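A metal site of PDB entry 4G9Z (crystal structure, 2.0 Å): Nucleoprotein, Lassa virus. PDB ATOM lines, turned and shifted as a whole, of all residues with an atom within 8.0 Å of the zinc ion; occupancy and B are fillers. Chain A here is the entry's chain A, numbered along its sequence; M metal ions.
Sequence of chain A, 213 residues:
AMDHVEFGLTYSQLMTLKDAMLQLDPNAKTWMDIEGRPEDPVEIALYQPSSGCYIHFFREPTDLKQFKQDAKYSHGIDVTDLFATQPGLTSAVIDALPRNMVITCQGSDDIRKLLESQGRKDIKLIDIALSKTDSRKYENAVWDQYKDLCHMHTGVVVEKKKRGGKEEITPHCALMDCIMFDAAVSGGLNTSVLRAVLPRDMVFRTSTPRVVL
OE2 of Glu 43 binds the zinc ion.
The zinc ion is bound by NE2 of His 153 (2.1 Å).
SG of Cys 173 binds the zinc ion.
The zinc ion is bound by the side-chain sulfur (SG) of Cys 150 (2.2 Å).
A ring nitrogen (ND1) of His 153 sits at hydrogen-bond distance from the backbone carbonyl oxygen (O) of His 75 (2.6 Å).
The side-chain sulfur (SG) of Cys 173 sits close to the backbone NH (N) of Met 176.
The side-chain carboxylate (OE1) of Glu 43 sits at hydrogen-bond distance from the backbone NH (N) of Ala 174 (2.8 Å).
The side-chain carboxylate (OE2) of Glu 43 sits close to a ring nitrogen (NE2) of His 56, 2.8 Å away.
The backbone NH (N) of Leu 175 sits close to the side-chain sulfur (SG) of Cys 173 (3.4 Å).
A ring nitrogen (ND1) of His 153 sits close to the backbone carbonyl oxygen (O) of His 172 (3.3 Å).
O of Glu 43 is in hydrogen-bond range of N of Glu 35, at 2.9 Å.
NE2 of His 56 touches the zinc ion, at 3.8 Å.
Along chain A the residues within 4 Å of the zinc ion span positions 43 to 173.
The nearest printed residue that does not touch the zinc ion is Ala 174 (4.2 Å).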
ATOM      1  N   GLU A  35      25.682 -29.474 -12.190  1.00  0.00           N
ATOM      2  CA  GLU A  35      27.033 -30.029 -12.092  1.00  0.00           C
ATOM      3  C   GLU A  35      27.150 -30.668 -10.737  1.00  0.00           C
ATOM      4  O   GLU A  35      26.514 -30.240  -9.770  1.00  0.00           O
ATOM      5  CB  GLU A  35      28.113 -28.955 -12.308  1.00  0.00           C
ATOM      6  CG  GLU A  35      28.102 -28.297 -13.673  1.00  0.00           C
ATOM      7  CD  GLU A  35      28.167 -29.300 -14.817  1.00  0.00           C
ATOM      8  OE1 GLU A  35      28.909 -30.295 -14.728  1.00  0.00           O
ATOM      9  OE2 GLU A  35      27.474 -29.085 -15.834  1.00  0.00           O
ATOM     10  N   GLU A  43      26.219 -27.352  -8.459  1.00  0.00           N
ATOM     11  CA  GLU A  43      25.723 -26.229  -9.256  1.00  0.00           C
ATOM     12  C   GLU A  43      24.387 -26.592  -9.911  1.00  0.00           C
ATOM     13  O   GLU A  43      24.268 -27.648 -10.512  1.00  0.00           O
ATOM     14  CB  GLU A  43      26.729 -25.801 -10.345  1.00  0.00           C
ATOM     15  CG  GLU A  43      26.288 -24.592 -11.174  1.00  0.00           C
ATOM     16  CD  GLU A  43      27.227 -24.201 -12.301  1.00  0.00           C
ATOM     17  OE1 GLU A  43      27.745 -25.095 -13.021  1.00  0.00           O
ATOM     18  OE2 GLU A  43      27.427 -22.989 -12.507  1.00  0.00           O
ATOM     19  N   ILE A  44      23.395 -25.718  -9.759  1.00  0.00           N
ATOM     20  CA  ILE A  44      22.063 -25.975 -10.295  1.00  0.00           C
ATOM     21  C   ILE A  44      21.586 -24.788 -11.116  1.00  0.00           C
ATOM     22  O   ILE A  44      21.774 -23.635 -10.715  1.00  0.00           O
ATOM     23  CB  ILE A  44      21.061 -26.330  -9.162  1.00  0.00           C
ATOM     24  CG1 ILE A  44      21.467 -27.661  -8.498  1.00  0.00           C
ATOM     25  CG2 ILE A  44      19.633 -26.379  -9.684  1.00  0.00           C
ATOM     26  CD1 ILE A  44      20.417 -28.279  -7.608  1.00  0.00           C
ATOM     27  N   ALA A  45      21.005 -25.073 -12.271  1.00  0.00           N
ATOM     28  CA  ALA A  45      20.447 -24.029 -13.110  1.00  0.00           C
ATOM     29  C   ALA A  45      19.147 -24.449 -13.758  1.00  0.00           C
ATOM     30  O   ALA A  45      18.996 -25.579 -14.167  1.00  0.00           O
ATOM     31  CB  ALA A  45      21.458 -23.610 -14.165  1.00  0.00           C
ATOM     32  N   HIS A  56      19.909 -19.849 -10.771  1.00  0.00           N
ATOM     33  CA  HIS A  56      21.290 -20.323 -10.780  1.00  0.00           C
ATOM     34  C   HIS A  56      21.871 -20.201  -9.393  1.00  0.00           C
ATOM     35  O   HIS A  56      21.887 -19.116  -8.797  1.00  0.00           O
ATOM     36  CB  HIS A  56      22.132 -19.533 -11.779  1.00  0.00           C
ATOM     37  CG  HIS A  56      23.550 -19.998 -11.898  1.00  0.00           C
ATOM     38  ND1 HIS A  56      24.604 -19.132 -11.972  1.00  0.00           N
ATOM     39  CD2 HIS A  56      24.079 -21.244 -11.941  1.00  0.00           C
ATOM     40  CE1 HIS A  56      25.737 -19.812 -12.078  1.00  0.00           C
ATOM     41  NE2 HIS A  56      25.439 -21.104 -12.053  1.00  0.00           N
ATOM     42  N   PHE A  57      22.339 -21.331  -8.853  1.00  0.00           N
ATOM     43  CA  PHE A  57      22.953 -21.312  -7.528  1.00  0.00           C
ATOM     44  C   PHE A  57      23.884 -22.499  -7.313  1.00  0.00           C
ATOM     45  O   PHE A  57      23.957 -23.410  -8.138  1.00  0.00           O
ATOM     46  CB  PHE A  57      21.887 -21.266  -6.428  1.00  0.00           C
ATOM     47  CG  PHE A  57      20.952 -22.443  -6.433  1.00  0.00           C
ATOM     48  CD1 PHE A  57      19.861 -22.465  -7.274  1.00  0.00           C
ATOM     49  CD2 PHE A  57      21.167 -23.519  -5.594  1.00  0.00           C
ATOM     50  CE1 PHE A  57      19.003 -23.555  -7.288  1.00  0.00           C
ATOM     51  CE2 PHE A  57      20.311 -24.603  -5.592  1.00  0.00           C
ATOM     52  CZ  PHE A  57      19.229 -24.618  -6.450  1.00  0.00           C
ATOM     53  N   PHE A  58      24.581 -22.468  -6.180  1.00  0.00           N
ATOM     54  CA  PHE A  58      25.619 -23.426  -5.885  1.00  0.00           C
ATOM     55  C   PHE A  58      25.402 -24.076  -4.527  1.00  0.00           C
ATOM     56  O   PHE A  58      24.586 -23.598  -3.741  1.00  0.00           O
ATOM     57  CB  PHE A  58      26.957 -22.697  -5.870  1.00  0.00           C
ATOM     58  CG  PHE A  58      27.357 -22.167  -7.208  1.00  0.00           C
ATOM     59  CD1 PHE A  58      28.052 -22.967  -8.096  1.00  0.00           C
ATOM     60  CD2 PHE A  58      27.025 -20.878  -7.585  1.00  0.00           C
ATOM     61  CE1 PHE A  58      28.420 -22.481  -9.348  1.00  0.00           C
ATOM     62  CE2 PHE A  58      27.371 -20.398  -8.839  1.00  0.00           C
ATOM     63  CZ  PHE A  58      28.088 -21.199  -9.704  1.00  0.00           C
ATOM     64  N   HIS A  75      33.706 -29.855 -14.358  1.00  0.00           N
ATOM     65  CA  HIS A  75      33.181 -28.508 -14.030  1.00  0.00           C
ATOM     66  C   HIS A  75      34.252 -27.498 -13.663  1.00  0.00           C
ATOM     67  O   HIS A  75      34.012 -26.304 -13.779  1.00  0.00           O
ATOM     68  CB  HIS A  75      32.053 -28.541 -12.971  1.00  0.00           C
ATOM     69  CG  HIS A  75      32.384 -29.281 -11.714  1.00  0.00           C
ATOM     70  ND1 HIS A  75      33.316 -28.837 -10.802  1.00  0.00           N
ATOM     71  CD2 HIS A  75      31.888 -30.434 -11.193  1.00  0.00           C
ATOM     72  CE1 HIS A  75      33.392 -29.677  -9.792  1.00  0.00           C
ATOM     73  NE2 HIS A  75      32.530 -30.658 -10.002  1.00  0.00           N
ATOM     74  N   ILE A  77      35.292 -26.362 -10.937  1.00  0.00           N
ATOM     75  CA  ILE A  77      35.005 -25.514  -9.781  1.00  0.00           C
ATOM     76  C   ILE A  77      36.015 -25.796  -8.664  1.00  0.00           C
ATOM     77  O   ILE A  77      36.290 -26.947  -8.330  1.00  0.00           O
ATOM     78  CB  ILE A  77      33.556 -25.710  -9.294  1.00  0.00           C
ATOM     79  CG1 ILE A  77      32.588 -25.501 -10.455  1.00  0.00           C
ATOM     80  CG2 ILE A  77      33.254 -24.756  -8.148  1.00  0.00           C
ATOM     81  CD1 ILE A  77      31.175 -25.955 -10.154  1.00  0.00           C
ATOM     82  N   TRP A 143      29.288 -18.978 -24.458  1.00  0.00           N
ATOM     83  CA  TRP A 143      30.286 -18.418 -23.559  1.00  0.00           C
ATOM     84  C   TRP A 143      30.701 -17.020 -23.996  1.00  0.00           C
ATOM     85  O   TRP A 143      30.895 -16.155 -23.147  1.00  0.00           O
ATOM     86  CB  TRP A 143      31.549 -19.285 -23.458  1.00  0.00           C
ATOM     87  CG  TRP A 143      31.440 -20.494 -22.591  1.00  0.00           C
ATOM     88  CD1 TRP A 143      31.211 -21.783 -22.998  1.00  0.00           C
ATOM     89  CD2 TRP A 143      31.577 -20.550 -21.160  1.00  0.00           C
ATOM     90  NE1 TRP A 143      31.194 -22.621 -21.927  1.00  0.00           N
ATOM     91  CE2 TRP A 143      31.408 -21.902 -20.781  1.00  0.00           C
ATOM     92  CE3 TRP A 143      31.806 -19.602 -20.162  1.00  0.00           C
ATOM     93  CZ2 TRP A 143      31.466 -22.322 -19.459  1.00  0.00           C
ATOM     94  CZ3 TRP A 143      31.860 -20.026 -18.832  1.00  0.00           C
ATOM     95  CH2 TRP A 143      31.702 -21.373 -18.493  1.00  0.00           C
ATOM     96  N   LYS A 147      29.445 -15.253 -20.636  1.00  0.00           N
ATOM     97  CA  LYS A 147      30.504 -15.566 -19.663  1.00  0.00           C
ATOM     98  C   LYS A 147      30.389 -14.808 -18.347  1.00  0.00           C
ATOM     99  O   LYS A 147      30.724 -15.364 -17.312  1.00  0.00           O
ATOM    100  CB  LYS A 147      31.907 -15.334 -20.280  1.00  0.00           C
ATOM    101  CG  LYS A 147      32.069 -13.996 -20.993  1.00  0.00           C
ATOM    102  CD  LYS A 147      33.398 -13.867 -21.727  1.00  0.00           C
ATOM    103  CE  LYS A 147      33.422 -12.653 -22.649  1.00  0.00           C
ATOM    104  NZ  LYS A 147      34.746 -12.418 -23.268  1.00  0.00           N
ATOM    105  N   LEU A 149      28.017 -14.251 -16.557  1.00  0.00           N
ATOM    106  CA  LEU A 149      26.979 -14.792 -15.700  1.00  0.00           C
ATOM    107  C   LEU A 149      27.462 -15.911 -14.776  1.00  0.00           C
ATOM    108  O   LEU A 149      26.768 -16.292 -13.841  1.00  0.00           O
ATOM    109  CB  LEU A 149      25.785 -15.267 -16.508  1.00  0.00           C
ATOM    110  CG  LEU A 149      25.077 -14.208 -17.347  1.00  0.00           C
ATOM    111  CD1 LEU A 149      23.911 -14.820 -18.102  1.00  0.00           C
ATOM    112  CD2 LEU A 149      24.609 -13.059 -16.470  1.00  0.00           C
ATOM    113  N   CYS A 150      28.655 -16.435 -15.037  1.00  0.00           N
ATOM    114  CA  CYS A 150      29.272 -17.435 -14.148  1.00  0.00           C
ATOM    115  C   CYS A 150      30.799 -17.391 -14.153  1.00  0.00           C
ATOM    116  O   CYS A 150      31.427 -17.560 -15.209  1.00  0.00           O
ATOM    117  CB  CYS A 150      28.821 -18.842 -14.529  1.00  0.00           C
ATOM    118  SG  CYS A 150      29.085 -20.047 -13.201  1.00  0.00           S
ATOM    119  N   HIS A 151      31.377 -17.176 -12.981  1.00  0.00           N
ATOM    120  CA  HIS A 151      32.817 -16.900 -12.826  1.00  0.00           C
ATOM    121  C   HIS A 151      33.494 -18.026 -12.044  1.00  0.00           C
ATOM    122  O   HIS A 151      34.604 -17.903 -11.499  1.00  0.00           O
ATOM    123  CB  HIS A 151      33.010 -15.592 -12.069  1.00  0.00           C
ATOM    124  CG  HIS A 151      32.526 -14.395 -12.817  1.00  0.00           C
ATOM    125  ND1 HIS A 151      33.376 -13.597 -13.543  1.00  0.00           N
ATOM    126  CD2 HIS A 151      31.284 -13.879 -12.982  1.00  0.00           C
ATOM    127  CE1 HIS A 151      32.683 -12.623 -14.109  1.00  0.00           C
ATOM    128  NE2 HIS A 151      31.415 -12.779 -13.787  1.00  0.00           N
ATOM    129  N   MET A 152      32.782 -19.125 -12.009  1.00  0.00           N
ATOM    130  CA  MET A 152      33.052 -20.203 -11.082  1.00  0.00           C
ATOM    131  C   MET A 152      33.916 -21.338 -11.662  1.00  0.00           C
ATOM    132  O   MET A 152      34.466 -22.139 -10.931  1.00  0.00           O
ATOM    133  CB  MET A 152      31.702 -20.704 -10.599  1.00  0.00           C
ATOM    134  CG  MET A 152      31.708 -21.679  -9.442  1.00  0.00           C
ATOM    135  SD  MET A 152      32.357 -21.070  -7.863  1.00  0.00           S
ATOM    136  CE  MET A 152      31.247 -19.751  -7.430  1.00  0.00           C
ATOM    137  N   HIS A 153      34.080 -21.400 -12.974  1.00  0.00           N
ATOM    138  CA  HIS A 153      34.807 -22.516 -13.558  1.00  0.00           C
ATOM    139  C   HIS A 153      36.200 -22.036 -13.930  1.00  0.00           C
ATOM    140  O   HIS A 153      36.485 -21.661 -15.056  1.00  0.00           O
ATOM    141  CB  HIS A 153      34.012 -23.061 -14.741  1.00  0.00           C
ATOM    142  CG  HIS A 153      32.568 -23.298 -14.400  1.00  0.00           C
ATOM    143  ND1 HIS A 153      32.100 -24.523 -13.979  1.00  0.00           N
ATOM    144  CD2 HIS A 153      31.501 -22.461 -14.376  1.00  0.00           C
ATOM    145  CE1 HIS A 153      30.806 -24.434 -13.713  1.00  0.00           C
ATOM    146  NE2 HIS A 153      30.426 -23.196 -13.956  1.00  0.00           N
ATOM    147  N   PRO A 171      35.340 -25.871 -19.582  1.00  0.00           N
ATOM    148  CA  PRO A 171      34.596 -26.374 -18.413  1.00  0.00           C
ATOM    149  C   PRO A 171      33.078 -26.438 -18.627  1.00  0.00           C
ATOM    150  O   PRO A 171      32.545 -25.668 -19.424  1.00  0.00           O
ATOM    151  CB  PRO A 171      34.926 -25.353 -17.319  1.00  0.00           C
ATOM    152  CG  PRO A 171      36.224 -24.770 -17.723  1.00  0.00           C
ATOM    153  CD  PRO A 171      36.183 -24.712 -19.223  1.00  0.00           C
ATOM    154  N   HIS A 172      32.431 -27.352 -17.916  1.00  0.00           N
ATOM    155  CA  HIS A 172      30.985 -27.517 -18.016  1.00  0.00           C
ATOM    156  C   HIS A 172      30.278 -26.698 -16.945  1.00  0.00           C
ATOM    157  O   HIS A 172      30.571 -26.882 -15.752  1.00  0.00           O
ATOM    158  CB  HIS A 172      30.592 -28.986 -18.019  1.00  0.00           C
ATOM    159  CG  HIS A 172      31.028 -29.719 -19.254  1.00  0.00           C
ATOM    160  ND1 HIS A 172      30.996 -31.088 -19.364  1.00  0.00           N
ATOM    161  CD2 HIS A 172      31.542 -29.255 -20.416  1.00  0.00           C
ATOM    162  CE1 HIS A 172      31.450 -31.445 -20.552  1.00  0.00           C
ATOM    163  NE2 HIS A 172      31.799 -30.353 -21.211  1.00  0.00           N
ATOM    164  N   CYS A 173      29.401 -25.799 -17.374  1.00  0.00           N
ATOM    165  CA  CYS A 173      28.633 -24.920 -16.490  1.00  0.00           C
ATOM    166  C   CYS A 173      27.144 -25.238 -16.653  1.00  0.00           C
ATOM    167  O   CYS A 173      26.646 -25.322 -17.764  1.00  0.00           O
ATOM    168  CB  CYS A 173      28.867 -23.448 -16.822  1.00  0.00           C
ATOM    169  SG  CYS A 173      27.739 -22.255 -16.005  1.00  0.00           S
ATOM    170  N   ALA A 174      26.447 -25.385 -15.525  1.00  0.00           N
ATOM    171  CA  ALA A 174      25.010 -25.708 -15.554  1.00  0.00           C
ATOM    172  C   ALA A 174      24.217 -24.659 -16.321  1.00  0.00           C
ATOM    173  O   ALA A 174      23.292 -24.983 -17.082  1.00  0.00           O
ATOM    174  CB  ALA A 174      24.483 -25.854 -14.133  1.00  0.00           C
ATOM    175  N   LEU A 175      24.551 -23.390 -16.119  1.00  0.00           N
ATOM    176  CA  LEU A 175      23.862 -22.300 -16.791  1.00  0.00           C
ATOM    177  C   LEU A 175      24.185 -22.248 -18.284  1.00  0.00           C
ATOM    178  O   LEU A 175      23.275 -22.219 -19.107  1.00  0.00           O
ATOM    179  CB  LEU A 175      24.157 -20.958 -16.098  1.00  0.00           C
ATOM    180  CG  LEU A 175      23.379 -19.747 -16.632  1.00  0.00           C
ATOM    181  CD1 LEU A 175      21.882 -19.992 -16.648  1.00  0.00           C
ATOM    182  CD2 LEU A 175      23.709 -18.506 -15.820  1.00  0.00           C
ATOM    183  N   MET A 176      25.469 -22.231 -18.632  1.00  0.00           N
ATOM    184  CA  MET A 176      25.844 -22.222 -20.044  1.00  0.00           C
ATOM    185  C   MET A 176      25.269 -23.442 -20.771  1.00  0.00           C
ATOM    186  O   MET A 176      24.825 -23.312 -21.910  1.00  0.00           O
ATOM    187  CB  MET A 176      27.376 -22.169 -20.224  1.00  0.00           C
ATOM    188  CG  MET A 176      28.071 -20.996 -19.562  1.00  0.00           C
ATOM    189  SD  MET A 176      27.310 -19.398 -19.901  1.00  0.00           S
ATOM    190  CE  MET A 176      27.706 -18.536 -18.384  1.00  0.00           C
ATOM    191  N   ASP A 177      25.258 -24.600 -20.108  1.00  0.00           N
ATOM    192  CA  ASP A 177      24.670 -25.802 -20.690  1.00  0.00           C
ATOM    193  C   ASP A 177      23.193 -25.578 -21.087  1.00  0.00           C
ATOM    194  O   ASP A 177      22.815 -25.867 -22.235  1.00  0.00           O
ATOM    195  CB  ASP A 177      24.807 -27.017 -19.769  1.00  0.00           C
ATOM    196  CG  ASP A 177      26.147 -27.724 -19.934  1.00  0.00           C
ATOM    197  OD1 ASP A 177      27.006 -27.236 -20.689  1.00  0.00           O
ATOM    198  OD2 ASP A 177      26.325 -28.783 -19.299  1.00  0.00           O
HETATM  199 ZN    ZN M   1      28.604 -22.091 -13.960  1.00  0.00          ZN
